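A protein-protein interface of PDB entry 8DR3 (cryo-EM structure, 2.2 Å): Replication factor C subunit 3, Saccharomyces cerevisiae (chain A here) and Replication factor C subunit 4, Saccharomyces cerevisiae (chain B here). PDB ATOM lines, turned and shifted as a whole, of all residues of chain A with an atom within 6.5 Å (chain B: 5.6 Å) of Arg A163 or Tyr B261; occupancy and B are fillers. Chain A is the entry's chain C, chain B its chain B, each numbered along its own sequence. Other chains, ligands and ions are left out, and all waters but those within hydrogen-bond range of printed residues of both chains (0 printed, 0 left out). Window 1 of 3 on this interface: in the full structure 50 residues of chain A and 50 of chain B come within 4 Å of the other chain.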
ATOM      1  N   HIS A  48      -1.246 -18.725 -21.063  1.00  0.00           N
ATOM      2  CA  HIS A  48      -2.635 -18.295 -20.989  1.00  0.00           C
ATOM      3  C   HIS A  48      -2.877 -17.204 -22.023  1.00  0.00           C
ATOM      4  O   HIS A  48      -2.097 -16.254 -22.134  1.00  0.00           O
ATOM      5  CB  HIS A  48      -2.968 -17.791 -19.583  1.00  0.00           C
ATOM      6  CG  HIS A  48      -2.558 -18.732 -18.492  1.00  0.00           C
ATOM      7  ND1 HIS A  48      -3.385 -19.729 -18.020  1.00  0.00           N
ATOM      8  CD2 HIS A  48      -1.411 -18.826 -17.779  1.00  0.00           C
ATOM      9  CE1 HIS A  48      -2.763 -20.398 -17.066  1.00  0.00           C
ATOM     10  NE2 HIS A  48      -1.565 -19.869 -16.900  1.00  0.00           N
ATOM     11  N   LEU A  49      -3.959 -17.339 -22.782  1.00  0.00           N
ATOM     12  CA  LEU A  49      -4.187 -16.523 -23.964  1.00  0.00           C
ATOM     13  C   LEU A  49      -5.405 -15.626 -23.789  1.00  0.00           C
ATOM     14  O   LEU A  49      -6.380 -15.992 -23.129  1.00  0.00           O
ATOM     15  CB  LEU A  49      -4.381 -17.404 -25.204  1.00  0.00           C
ATOM     16  CG  LEU A  49      -3.182 -18.237 -25.661  1.00  0.00           C
ATOM     17  CD1 LEU A  49      -3.526 -18.998 -26.930  1.00  0.00           C
ATOM     18  CD2 LEU A  49      -1.956 -17.364 -25.878  1.00  0.00           C
ATOM     19  N   LEU A  50      -5.333 -14.443 -24.394  1.00  0.00           N
ATOM     20  CA  LEU A  50      -6.469 -13.543 -24.526  1.00  0.00           C
ATOM     21  C   LEU A  50      -6.574 -13.139 -25.987  1.00  0.00           C
ATOM     22  O   LEU A  50      -5.575 -12.748 -26.594  1.00  0.00           O
ATOM     23  CB  LEU A  50      -6.308 -12.305 -23.635  1.00  0.00           C
ATOM     24  CG  LEU A  50      -7.263 -11.136 -23.901  1.00  0.00           C
ATOM     25  CD1 LEU A  50      -8.712 -11.567 -23.728  1.00  0.00           C
ATOM     26  CD2 LEU A  50      -6.941  -9.967 -22.988  1.00  0.00           C
ATOM     27  N   PHE A  51      -7.772 -13.254 -26.553  1.00  0.00           N
ATOM     28  CA  PHE A  51      -8.052 -12.877 -27.935  1.00  0.00           C
ATOM     29  C   PHE A  51      -9.054 -11.733 -27.903  1.00  0.00           C
ATOM     30  O   PHE A  51     -10.235 -11.946 -27.605  1.00  0.00           O
ATOM     31  CB  PHE A  51      -8.604 -14.058 -28.736  1.00  0.00           C
ATOM     32  CG  PHE A  51      -7.587 -15.127 -29.057  1.00  0.00           C
ATOM     33  CD1 PHE A  51      -6.250 -14.979 -28.722  1.00  0.00           C
ATOM     34  CD2 PHE A  51      -7.982 -16.287 -29.705  1.00  0.00           C
ATOM     35  CE1 PHE A  51      -5.331 -15.966 -29.025  1.00  0.00           C
ATOM     36  CE2 PHE A  51      -7.066 -17.277 -30.010  1.00  0.00           C
ATOM     37  CZ  PHE A  51      -5.739 -17.115 -29.669  1.00  0.00           C
ATOM     38  N   TYR A  52      -8.591 -10.526 -28.211  1.00  0.00           N
ATOM     39  CA  TYR A  52      -9.433  -9.337 -28.204  1.00  0.00           C
ATOM     40  C   TYR A  52      -9.650  -8.870 -29.635  1.00  0.00           C
ATOM     41  O   TYR A  52      -8.684  -8.679 -30.378  1.00  0.00           O
ATOM     42  CB  TYR A  52      -8.797  -8.222 -27.371  1.00  0.00           C
ATOM     43  CG  TYR A  52      -9.497  -6.890 -27.499  1.00  0.00           C
ATOM     44  CD1 TYR A  52     -10.662  -6.624 -26.791  1.00  0.00           C
ATOM     45  CD2 TYR A  52      -8.993  -5.896 -28.326  1.00  0.00           C
ATOM     46  CE1 TYR A  52     -11.304  -5.407 -26.905  1.00  0.00           C
ATOM     47  CE2 TYR A  52      -9.629  -4.675 -28.445  1.00  0.00           C
ATOM     48  CZ  TYR A  52     -10.784  -4.436 -27.733  1.00  0.00           C
ATOM     49  OH  TYR A  52     -11.419  -3.222 -27.851  1.00  0.00           O
ATOM     50  N   PRO A  54     -12.906  -7.278 -32.780  1.00  0.00           N
ATOM     51  CA  PRO A  54     -14.280  -6.912 -33.142  1.00  0.00           C
ATOM     52  C   PRO A  54     -15.033  -8.095 -33.724  1.00  0.00           C
ATOM     53  O   PRO A  54     -14.441  -9.152 -33.989  1.00  0.00           O
ATOM     54  CB  PRO A  54     -14.085  -5.802 -34.185  1.00  0.00           C
ATOM     55  CG  PRO A  54     -12.764  -6.086 -34.796  1.00  0.00           C
ATOM     56  CD  PRO A  54     -11.921  -6.762 -33.747  1.00  0.00           C
ATOM     57  N   ASN A 148     -14.662  -8.911 -27.021  1.00  0.00           N
ATOM     58  CA  ASN A 148     -14.816  -7.762 -27.903  1.00  0.00           C
ATOM     59  C   ASN A 148     -14.602  -6.439 -27.181  1.00  0.00           C
ATOM     60  O   ASN A 148     -14.212  -5.455 -27.817  1.00  0.00           O
ATOM     61  CB  ASN A 148     -16.215  -7.755 -28.533  1.00  0.00           C
ATOM     62  CG  ASN A 148     -16.491  -8.991 -29.368  1.00  0.00           C
ATOM     63  OD1 ASN A 148     -17.353  -9.799 -29.031  1.00  0.00           O
ATOM     64  ND2 ASN A 148     -15.768  -9.136 -30.470  1.00  0.00           N
ATOM     65  N   ALA A 150     -12.604  -4.806 -23.945  1.00  0.00           N
ATOM     66  CA  ALA A 150     -11.591  -5.058 -22.926  1.00  0.00           C
ATOM     67  C   ALA A 150     -11.952  -4.421 -21.591  1.00  0.00           C
ATOM     68  O   ALA A 150     -11.499  -4.892 -20.541  1.00  0.00           O
ATOM     69  CB  ALA A 150     -10.233  -4.546 -23.404  1.00  0.00           C
ATOM     70  N   LEU A 158      -6.398  -9.603 -16.730  1.00  0.00           N
ATOM     71  CA  LEU A 158      -5.548  -9.194 -17.843  1.00  0.00           C
ATOM     72  C   LEU A 158      -4.072  -9.362 -17.507  1.00  0.00           C
ATOM     73  O   LEU A 158      -3.257  -9.621 -18.400  1.00  0.00           O
ATOM     74  CB  LEU A 158      -5.842  -7.742 -18.221  1.00  0.00           C
ATOM     75  CG  LEU A 158      -7.187  -7.484 -18.905  1.00  0.00           C
ATOM     76  CD1 LEU A 158      -7.719  -6.107 -18.535  1.00  0.00           C
ATOM     77  CD2 LEU A 158      -7.068  -7.626 -20.412  1.00  0.00           C
ATOM     78  N   CYS A 161      -2.616 -12.932 -18.542  1.00  0.00           N
ATOM     79  CA  CYS A 161      -2.837 -13.443 -19.886  1.00  0.00           C
ATOM     80  C   CYS A 161      -1.952 -12.715 -20.889  1.00  0.00           C
ATOM     81  O   CYS A 161      -1.607 -11.545 -20.706  1.00  0.00           O
ATOM     82  CB  CYS A 161      -4.309 -13.296 -20.305  1.00  0.00           C
ATOM     83  SG  CYS A 161      -5.473 -14.260 -19.313  1.00  0.00           S
ATOM     84  N   THR A 162      -1.590 -13.428 -21.953  1.00  0.00           N
ATOM     85  CA  THR A 162      -0.873 -12.846 -23.081  1.00  0.00           C
ATOM     86  C   THR A 162      -1.886 -12.439 -24.144  1.00  0.00           C
ATOM     87  O   THR A 162      -2.706 -13.255 -24.573  1.00  0.00           O
ATOM     88  CB  THR A 162       0.137 -13.840 -23.657  1.00  0.00           C
ATOM     89  OG1 THR A 162       1.098 -14.185 -22.652  1.00  0.00           O
ATOM     90  CG2 THR A 162       0.858 -13.242 -24.857  1.00  0.00           C
ATOM     91  N   ARG A 163      -1.823 -11.179 -24.565  1.00  0.00           N
ATOM     92  CA  ARG A 163      -2.877 -10.559 -25.357  1.00  0.00           C
ATOM     93  C   ARG A 163      -2.559 -10.645 -26.844  1.00  0.00           C
ATOM     94  O   ARG A 163      -1.426 -10.385 -27.261  1.00  0.00           O
ATOM     95  CB  ARG A 163      -3.061  -9.098 -24.941  1.00  0.00           C
ATOM     96  CG  ARG A 163      -4.050  -8.315 -25.790  1.00  0.00           C
ATOM     97  CD  ARG A 163      -4.379  -6.976 -25.145  1.00  0.00           C
ATOM     98  NE  ARG A 163      -5.327  -6.197 -25.935  1.00  0.00           N
ATOM     99  CZ  ARG A 163      -4.997  -5.437 -26.970  1.00  0.00           C
ATOM    100  NH1 ARG A 163      -3.744  -5.329 -27.381  1.00  0.00           N
ATOM    101  NH2 ARG A 163      -5.951  -4.766 -27.611  1.00  0.00           N
ATOM    102  N   PHE A 164      -3.567 -11.009 -27.637  1.00  0.00           N
ATOM    103  CA  PHE A 164      -3.493 -11.018 -29.090  1.00  0.00           C
ATOM    104  C   PHE A 164      -4.696 -10.261 -29.630  1.00  0.00           C
ATOM    105  O   PHE A 164      -5.841 -10.572 -29.274  1.00  0.00           O
ATOM    106  CB  PHE A 164      -3.477 -12.447 -29.642  1.00  0.00           C
ATOM    107  CG  PHE A 164      -2.176 -13.167 -29.435  1.00  0.00           C
ATOM    108  CD1 PHE A 164      -1.123 -12.991 -30.316  1.00  0.00           C
ATOM    109  CD2 PHE A 164      -2.010 -14.027 -28.362  1.00  0.00           C
ATOM    110  CE1 PHE A 164       0.074 -13.655 -30.129  1.00  0.00           C
ATOM    111  CE2 PHE A 164      -0.814 -14.693 -28.170  1.00  0.00           C
ATOM    112  CZ  PHE A 164       0.228 -14.507 -29.055  1.00  0.00           C
ATOM    113  N   ARG A 165      -4.439  -9.285 -30.493  1.00  0.00           N
ATOM    114  CA  ARG A 165      -5.479  -8.437 -31.057  1.00  0.00           C
ATOM    115  C   ARG A 165      -5.801  -8.911 -32.468  1.00  0.00           C
ATOM    116  O   ARG A 165      -4.906  -9.017 -33.313  1.00  0.00           O
ATOM    117  CB  ARG A 165      -5.040  -6.973 -31.065  1.00  0.00           C
ATOM    118  CG  ARG A 165      -5.986  -6.037 -31.804  1.00  0.00           C
ATOM    119  CD  ARG A 165      -5.547  -4.587 -31.674  1.00  0.00           C
ATOM    120  NE  ARG A 165      -4.156  -4.400 -32.068  1.00  0.00           N
ATOM    121  CZ  ARG A 165      -3.734  -4.321 -33.322  1.00  0.00           C
ATOM    122  NH1 ARG A 165      -4.571  -4.410 -34.342  1.00  0.00           N
ATOM    123  NH2 ARG A 165      -2.436  -4.152 -33.560  1.00  0.00           N
ATOM    124  N   PRO A 168      -9.374  -5.901 -38.014  1.00  0.00           N
ATOM    125  CA  PRO A 168     -10.365  -6.038 -39.087  1.00  0.00           C
ATOM    126  C   PRO A 168      -9.732  -6.676 -40.314  1.00  0.00           C
ATOM    127  O   PRO A 168      -8.596  -6.369 -40.679  1.00  0.00           O
ATOM    128  CB  PRO A 168     -10.813  -4.596 -39.358  1.00  0.00           C
ATOM    129  CG  PRO A 168     -10.383  -3.805 -38.177  1.00  0.00           C
ATOM    130  CD  PRO A 168      -9.230  -4.512 -37.547  1.00  0.00           C
ATOM    131  N   ILE B 227       4.885  -8.610 -29.760  1.00  0.00           N
ATOM    132  CA  ILE B 227       4.185  -9.423 -28.770  1.00  0.00           C
ATOM    133  C   ILE B 227       3.328  -8.552 -27.860  1.00  0.00           C
ATOM    134  O   ILE B 227       2.189  -8.908 -27.538  1.00  0.00           O
ATOM    135  CB  ILE B 227       5.196 -10.263 -27.968  1.00  0.00           C
ATOM    136  CG1 ILE B 227       5.605 -11.500 -28.773  1.00  0.00           C
ATOM    137  CG2 ILE B 227       4.616 -10.666 -26.616  1.00  0.00           C
ATOM    138  CD1 ILE B 227       4.593 -12.630 -28.726  1.00  0.00           C
ATOM    139  N   ASP B 229       1.396  -5.113 -27.434  1.00  0.00           N
ATOM    140  CA  ASP B 229       0.864  -3.952 -28.130  1.00  0.00           C
ATOM    141  C   ASP B 229       1.052  -2.695 -27.288  1.00  0.00           C
ATOM    142  O   ASP B 229       1.014  -2.734 -26.055  1.00  0.00           O
ATOM    143  CB  ASP B 229      -0.619  -4.152 -28.446  1.00  0.00           C
ATOM    144  CG  ASP B 229      -0.947  -3.883 -29.900  1.00  0.00           C
ATOM    145  OD1 ASP B 229      -0.382  -2.929 -30.475  1.00  0.00           O
ATOM    146  OD2 ASP B 229      -1.773  -4.627 -30.470  1.00  0.00           O
ATOM    147  N   SER B 230       1.261  -1.574 -27.966  1.00  0.00           N
ATOM    148  CA  SER B 230       1.393  -0.305 -27.266  1.00  0.00           C
ATOM    149  C   SER B 230       0.088   0.007 -26.537  1.00  0.00           C
ATOM    150  O   SER B 230      -0.986  -0.060 -27.150  1.00  0.00           O
ATOM    151  CB  SER B 230       1.734   0.816 -28.248  1.00  0.00           C
ATOM    152  OG  SER B 230       0.640   1.096 -29.106  1.00  0.00           O
ATOM    153  N   HIS B 232      -3.250   1.350 -25.373  1.00  0.00           N
ATOM    154  CA  HIS B 232      -4.159   2.289 -26.018  1.00  0.00           C
ATOM    155  C   HIS B 232      -4.434   3.538 -25.179  1.00  0.00           C
ATOM    156  O   HIS B 232      -4.812   4.567 -25.753  1.00  0.00           O
ATOM    157  CB  HIS B 232      -5.478   1.603 -26.405  1.00  0.00           C
ATOM    158  CG  HIS B 232      -6.269   1.071 -25.251  1.00  0.00           C
ATOM    159  ND1 HIS B 232      -7.520   1.548 -24.928  1.00  0.00           N
ATOM    160  CD2 HIS B 232      -6.022   0.054 -24.392  1.00  0.00           C
ATOM    161  CE1 HIS B 232      -7.989   0.882 -23.889  1.00  0.00           C
ATOM    162  NE2 HIS B 232      -7.099  -0.032 -23.544  1.00  0.00           N
ATOM    163  N   ASP B 255      -4.971   4.731 -35.541  1.00  0.00           N
ATOM    164  CA  ASP B 255      -4.371   3.989 -34.441  1.00  0.00           C
ATOM    165  C   ASP B 255      -5.389   3.288 -33.552  1.00  0.00           C
ATOM    166  O   ASP B 255      -5.004   2.396 -32.786  1.00  0.00           O
ATOM    167  CB  ASP B 255      -3.515   4.926 -33.585  1.00  0.00           C
ATOM    168  CG  ASP B 255      -2.465   5.656 -34.397  1.00  0.00           C
ATOM    169  OD1 ASP B 255      -1.744   4.991 -35.169  1.00  0.00           O
ATOM    170  OD2 ASP B 255      -2.361   6.893 -34.266  1.00  0.00           O
ATOM    171  N   LEU B 256      -6.664   3.667 -33.617  1.00  0.00           N
ATOM    172  CA  LEU B 256      -7.684   3.064 -32.768  1.00  0.00           C
ATOM    173  C   LEU B 256      -8.781   2.366 -33.555  1.00  0.00           C
ATOM    174  O   LEU B 256      -9.044   1.180 -33.321  1.00  0.00           O
ATOM    175  CB  LEU B 256      -8.296   4.137 -31.852  1.00  0.00           C
ATOM    176  CG  LEU B 256      -7.300   4.824 -30.914  1.00  0.00           C
ATOM    177  CD1 LEU B 256      -7.865   6.130 -30.376  1.00  0.00           C
ATOM    178  CD2 LEU B 256      -6.912   3.895 -29.774  1.00  0.00           C
ATOM    179  N   TRP B 257      -9.426   3.060 -34.496  1.00  0.00           N
ATOM    180  CA  TRP B 257     -10.604   2.494 -35.146  1.00  0.00           C
ATOM    181  C   TRP B 257     -10.226   1.386 -36.122  1.00  0.00           C
ATOM    182  O   TRP B 257     -10.869   0.330 -36.149  1.00  0.00           O
ATOM    183  CB  TRP B 257     -11.386   3.596 -35.859  1.00  0.00           C
ATOM    184  CG  TRP B 257     -12.685   3.125 -36.429  1.00  0.00           C
ATOM    185  CD1 TRP B 257     -12.931   2.765 -37.721  1.00  0.00           C
ATOM    186  CD2 TRP B 257     -13.918   2.956 -35.723  1.00  0.00           C
ATOM    187  NE1 TRP B 257     -14.244   2.385 -37.864  1.00  0.00           N
ATOM    188  CE2 TRP B 257     -14.871   2.492 -36.651  1.00  0.00           C
ATOM    189  CE3 TRP B 257     -14.310   3.152 -34.394  1.00  0.00           C
ATOM    190  CZ2 TRP B 257     -16.190   2.223 -36.295  1.00  0.00           C
ATOM    191  CZ3 TRP B 257     -15.620   2.884 -34.043  1.00  0.00           C
ATOM    192  CH2 TRP B 257     -16.544   2.425 -34.989  1.00  0.00           C
ATOM    193  N   LYS B 259      -7.606  -0.445 -35.984  1.00  0.00           N
ATOM    194  CA  LYS B 259      -6.974  -1.558 -35.289  1.00  0.00           C
ATOM    195  C   LYS B 259      -7.981  -2.502 -34.647  1.00  0.00           C
ATOM    196  O   LYS B 259      -7.580  -3.555 -34.143  1.00  0.00           O
ATOM    197  CB  LYS B 259      -6.011  -1.035 -34.221  1.00  0.00           C
ATOM    198  CG  LYS B 259      -5.013  -0.001 -34.723  1.00  0.00           C
ATOM    199  CD  LYS B 259      -4.120  -0.559 -35.831  1.00  0.00           C
ATOM    200  CE  LYS B 259      -2.642  -0.565 -35.451  1.00  0.00           C
ATOM    201  NZ  LYS B 259      -2.191   0.680 -34.768  1.00  0.00           N
ATOM    202  N   GLY B 260      -9.265  -2.157 -34.653  1.00  0.00           N
ATOM    203  CA  GLY B 260     -10.295  -3.015 -34.110  1.00  0.00           C
ATOM    204  C   GLY B 260     -10.757  -2.684 -32.709  1.00  0.00           C
ATOM    205  O   GLY B 260     -11.541  -3.452 -32.141  1.00  0.00           O
ATOM    206  N   TYR B 261     -10.298  -1.577 -32.129  1.00  0.00           N
ATOM    207  CA  TYR B 261     -10.757  -1.184 -30.804  1.00  0.00           C
ATOM    208  C   TYR B 261     -12.216  -0.748 -30.861  1.00  0.00           C
ATOM    209  O   TYR B 261     -12.616   0.010 -31.751  1.00  0.00           O
ATOM    210  CB  TYR B 261      -9.885  -0.058 -30.253  1.00  0.00           C
ATOM    211  CG  TYR B 261      -8.491  -0.501 -29.870  1.00  0.00           C
ATOM    212  CD1 TYR B 261      -8.244  -1.094 -28.639  1.00  0.00           C
ATOM    213  CD2 TYR B 261      -7.423  -0.329 -30.740  1.00  0.00           C
ATOM    214  CE1 TYR B 261      -6.973  -1.503 -28.285  1.00  0.00           C
ATOM    215  CE2 TYR B 261      -6.148  -0.735 -30.395  1.00  0.00           C
ATOM    216  CZ  TYR B 261      -5.929  -1.321 -29.166  1.00  0.00           C
ATOM    217  OH  TYR B 261      -4.663  -1.726 -28.815  1.00  0.00           O
ATOM    218  N   SER B 262     -13.012  -1.227 -29.910  1.00  0.00           N
ATOM    219  CA  SER B 262     -14.431  -0.911 -29.886  1.00  0.00           C
ATOM    220  C   SER B 262     -14.658   0.530 -29.434  1.00  0.00           C
ATOM    221  O   SER B 262     -13.838   1.132 -28.735  1.00  0.00           O
ATOM    222  CB  SER B 262     -15.179  -1.875 -28.964  1.00  0.00           C
ATOM    223  OG  SER B 262     -14.689  -1.798 -27.638  1.00  0.00           O
ATOM    224  N   SER B 263     -15.801   1.083 -29.846  1.00  0.00           N
ATOM    225  CA  SER B 263     -16.128   2.461 -29.492  1.00  0.00           C
ATOM    226  C   SER B 263     -16.318   2.618 -27.987  1.00  0.00           C
ATOM    227  O   SER B 263     -15.915   3.634 -27.407  1.00  0.00           O
ATOM    228  CB  SER B 263     -17.382   2.910 -30.244  1.00  0.00           C
ATOM    229  OG  SER B 263     -18.511   2.140 -29.870  1.00  0.00           O
ATOM    230  N   ASP B 265     -14.841   0.928 -25.596  1.00  0.00           N
ATOM    231  CA  ASP B 265     -13.513   0.965 -24.996  1.00  0.00           C
ATOM    232  C   ASP B 265     -12.859   2.324 -25.207  1.00  0.00           C
ATOM    233  O   ASP B 265     -12.257   2.884 -24.282  1.00  0.00           O
ATOM    234  CB  ASP B 265     -12.641  -0.145 -25.583  1.00  0.00           C
ATOM    235  CG  ASP B 265     -12.896  -1.498 -24.939  1.00  0.00           C
ATOM    236  OD1 ASP B 265     -13.439  -1.537 -23.817  1.00  0.00           O
ATOM    237  OD2 ASP B 265     -12.551  -2.525 -25.557  1.00  0.00           O
ATOM    238  N   ILE B 266     -12.978   2.875 -26.416  1.00  0.00           N
ATOM    239  CA  ILE B 266     -12.359   4.163 -26.716  1.00  0.00           C
ATOM    240  C   ILE B 266     -12.938   5.252 -25.822  1.00  0.00           C
ATOM    241  O   ILE B 266     -12.202   6.066 -25.254  1.00  0.00           O
ATOM    242  CB  ILE B 266     -12.531   4.508 -28.207  1.00  0.00           C
ATOM    243  CG1 ILE B 266     -11.698   3.560 -29.072  1.00  0.00           C
ATOM    244  CG2 ILE B 266     -12.138   5.957 -28.470  1.00  0.00           C
ATOM    245  CD1 ILE B 266     -12.132   3.510 -30.519  1.00  0.00           C
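O of Lys B259 lies within hydrogen-bond range of NH1 of Arg A165, 3.1 Å away.
The backbone NH (N) of Ser B262 lies within hydrogen-bond range of the side-chain hydroxyl (OH) of Tyr A52 (3.3 Å).
The side-chain hydroxyl (OH) of Tyr A52 sits at hydrogen-bond distance from the side-chain carboxylate (OD2) of Asp B265 (2.7 Å).
The side-chain carboxylate (OD2) of Asp B265 lies within hydrogen-bond range of the backbone NH (N) of Ala A150.
The guanidinium group (NH1) of Arg A163 lies within salt-bridge range of the side-chain carboxylate (OD2) of Asp B229.
The guanidinium group (NE) of Arg A165 is in salt-bridge range of the side-chain carboxylate (OD2) of Asp B229 (2.9 Å).
The backbone carbonyl oxygen (O) of Leu B256 lies within hydrogen-bond range of the backbone NH (N) of Tyr B261, at 3.3 Å.
The backbone carbonyl oxygen (O) of Phe A164 lies within hydrogen-bond range of the backbone NH (N) of Tyr A52 (2.9 Å).
OG of Ser B262 is in hydrogen-bond range of OD2 of Asp B265 (3.1 Å).
Among the printed residues, merely in contact across the chains: Tyr A52 with Tyr B261 (3.6 Å), Pro A54 with Gly B260 (3.7 Å), Asn A148 with Ser B262 (3.7 Å), Arg A163 with Ile B227 (3.9 Å), Arg A163 with Tyr B261 (3.5 Å), Pro A168 with Lys B259 (3.7 Å) and Pro A168 with Gly B260 (3.7 Å).
Printed residues of chain B within 4 Å of Ala A150: Asp B265 (2.8 Å).
Arg A163 touches just these residues of chain B: Ile B227 (3.9 Å), Asp B229 (3.5 Å) and Tyr B261 (3.5 Å).
Phe A164 touches none of the printed residues of chain B.
Of the printed residues of chain A, Ile B227 touches Arg A163.
Of the printed residues of chain A, Gly B260 touches Pro A54 (3.7 Å) and Pro A168 (3.7 Å).
Tyr B261 touches two residues of chain A.
Ile B266 touches none of the printed residues of chain A.
The nearest printed residue of chain B that does not touch Arg A163 is His B232 (5.8 Å).
Hydrophobic or aromatic side chains of chain B that line the printed part of chain A: Tyr B261.
Of the 15 printed residues of chain A, 7 touch a printed residue of chain B.
Printed residues of chain A that touch a printed residue of chain B: Tyr A52, Pro A54, Asn A148, Ala A150, Arg A163, Arg A165 and Pro A168.
Hydrophobic or aromatic side chains of chain A that line the printed part of chain B: Tyr A52, Pro A54, Ala A150 and Pro A168.
Among the printed residues, 13 pairs touch across the chains.
Among the printed residues, Asp or Glu carboxylates within 4 Å of a Lys or Arg side-chain nitrogen of the other chain: Arg A163 with Asp B229 and Arg A165 with Asp B229.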
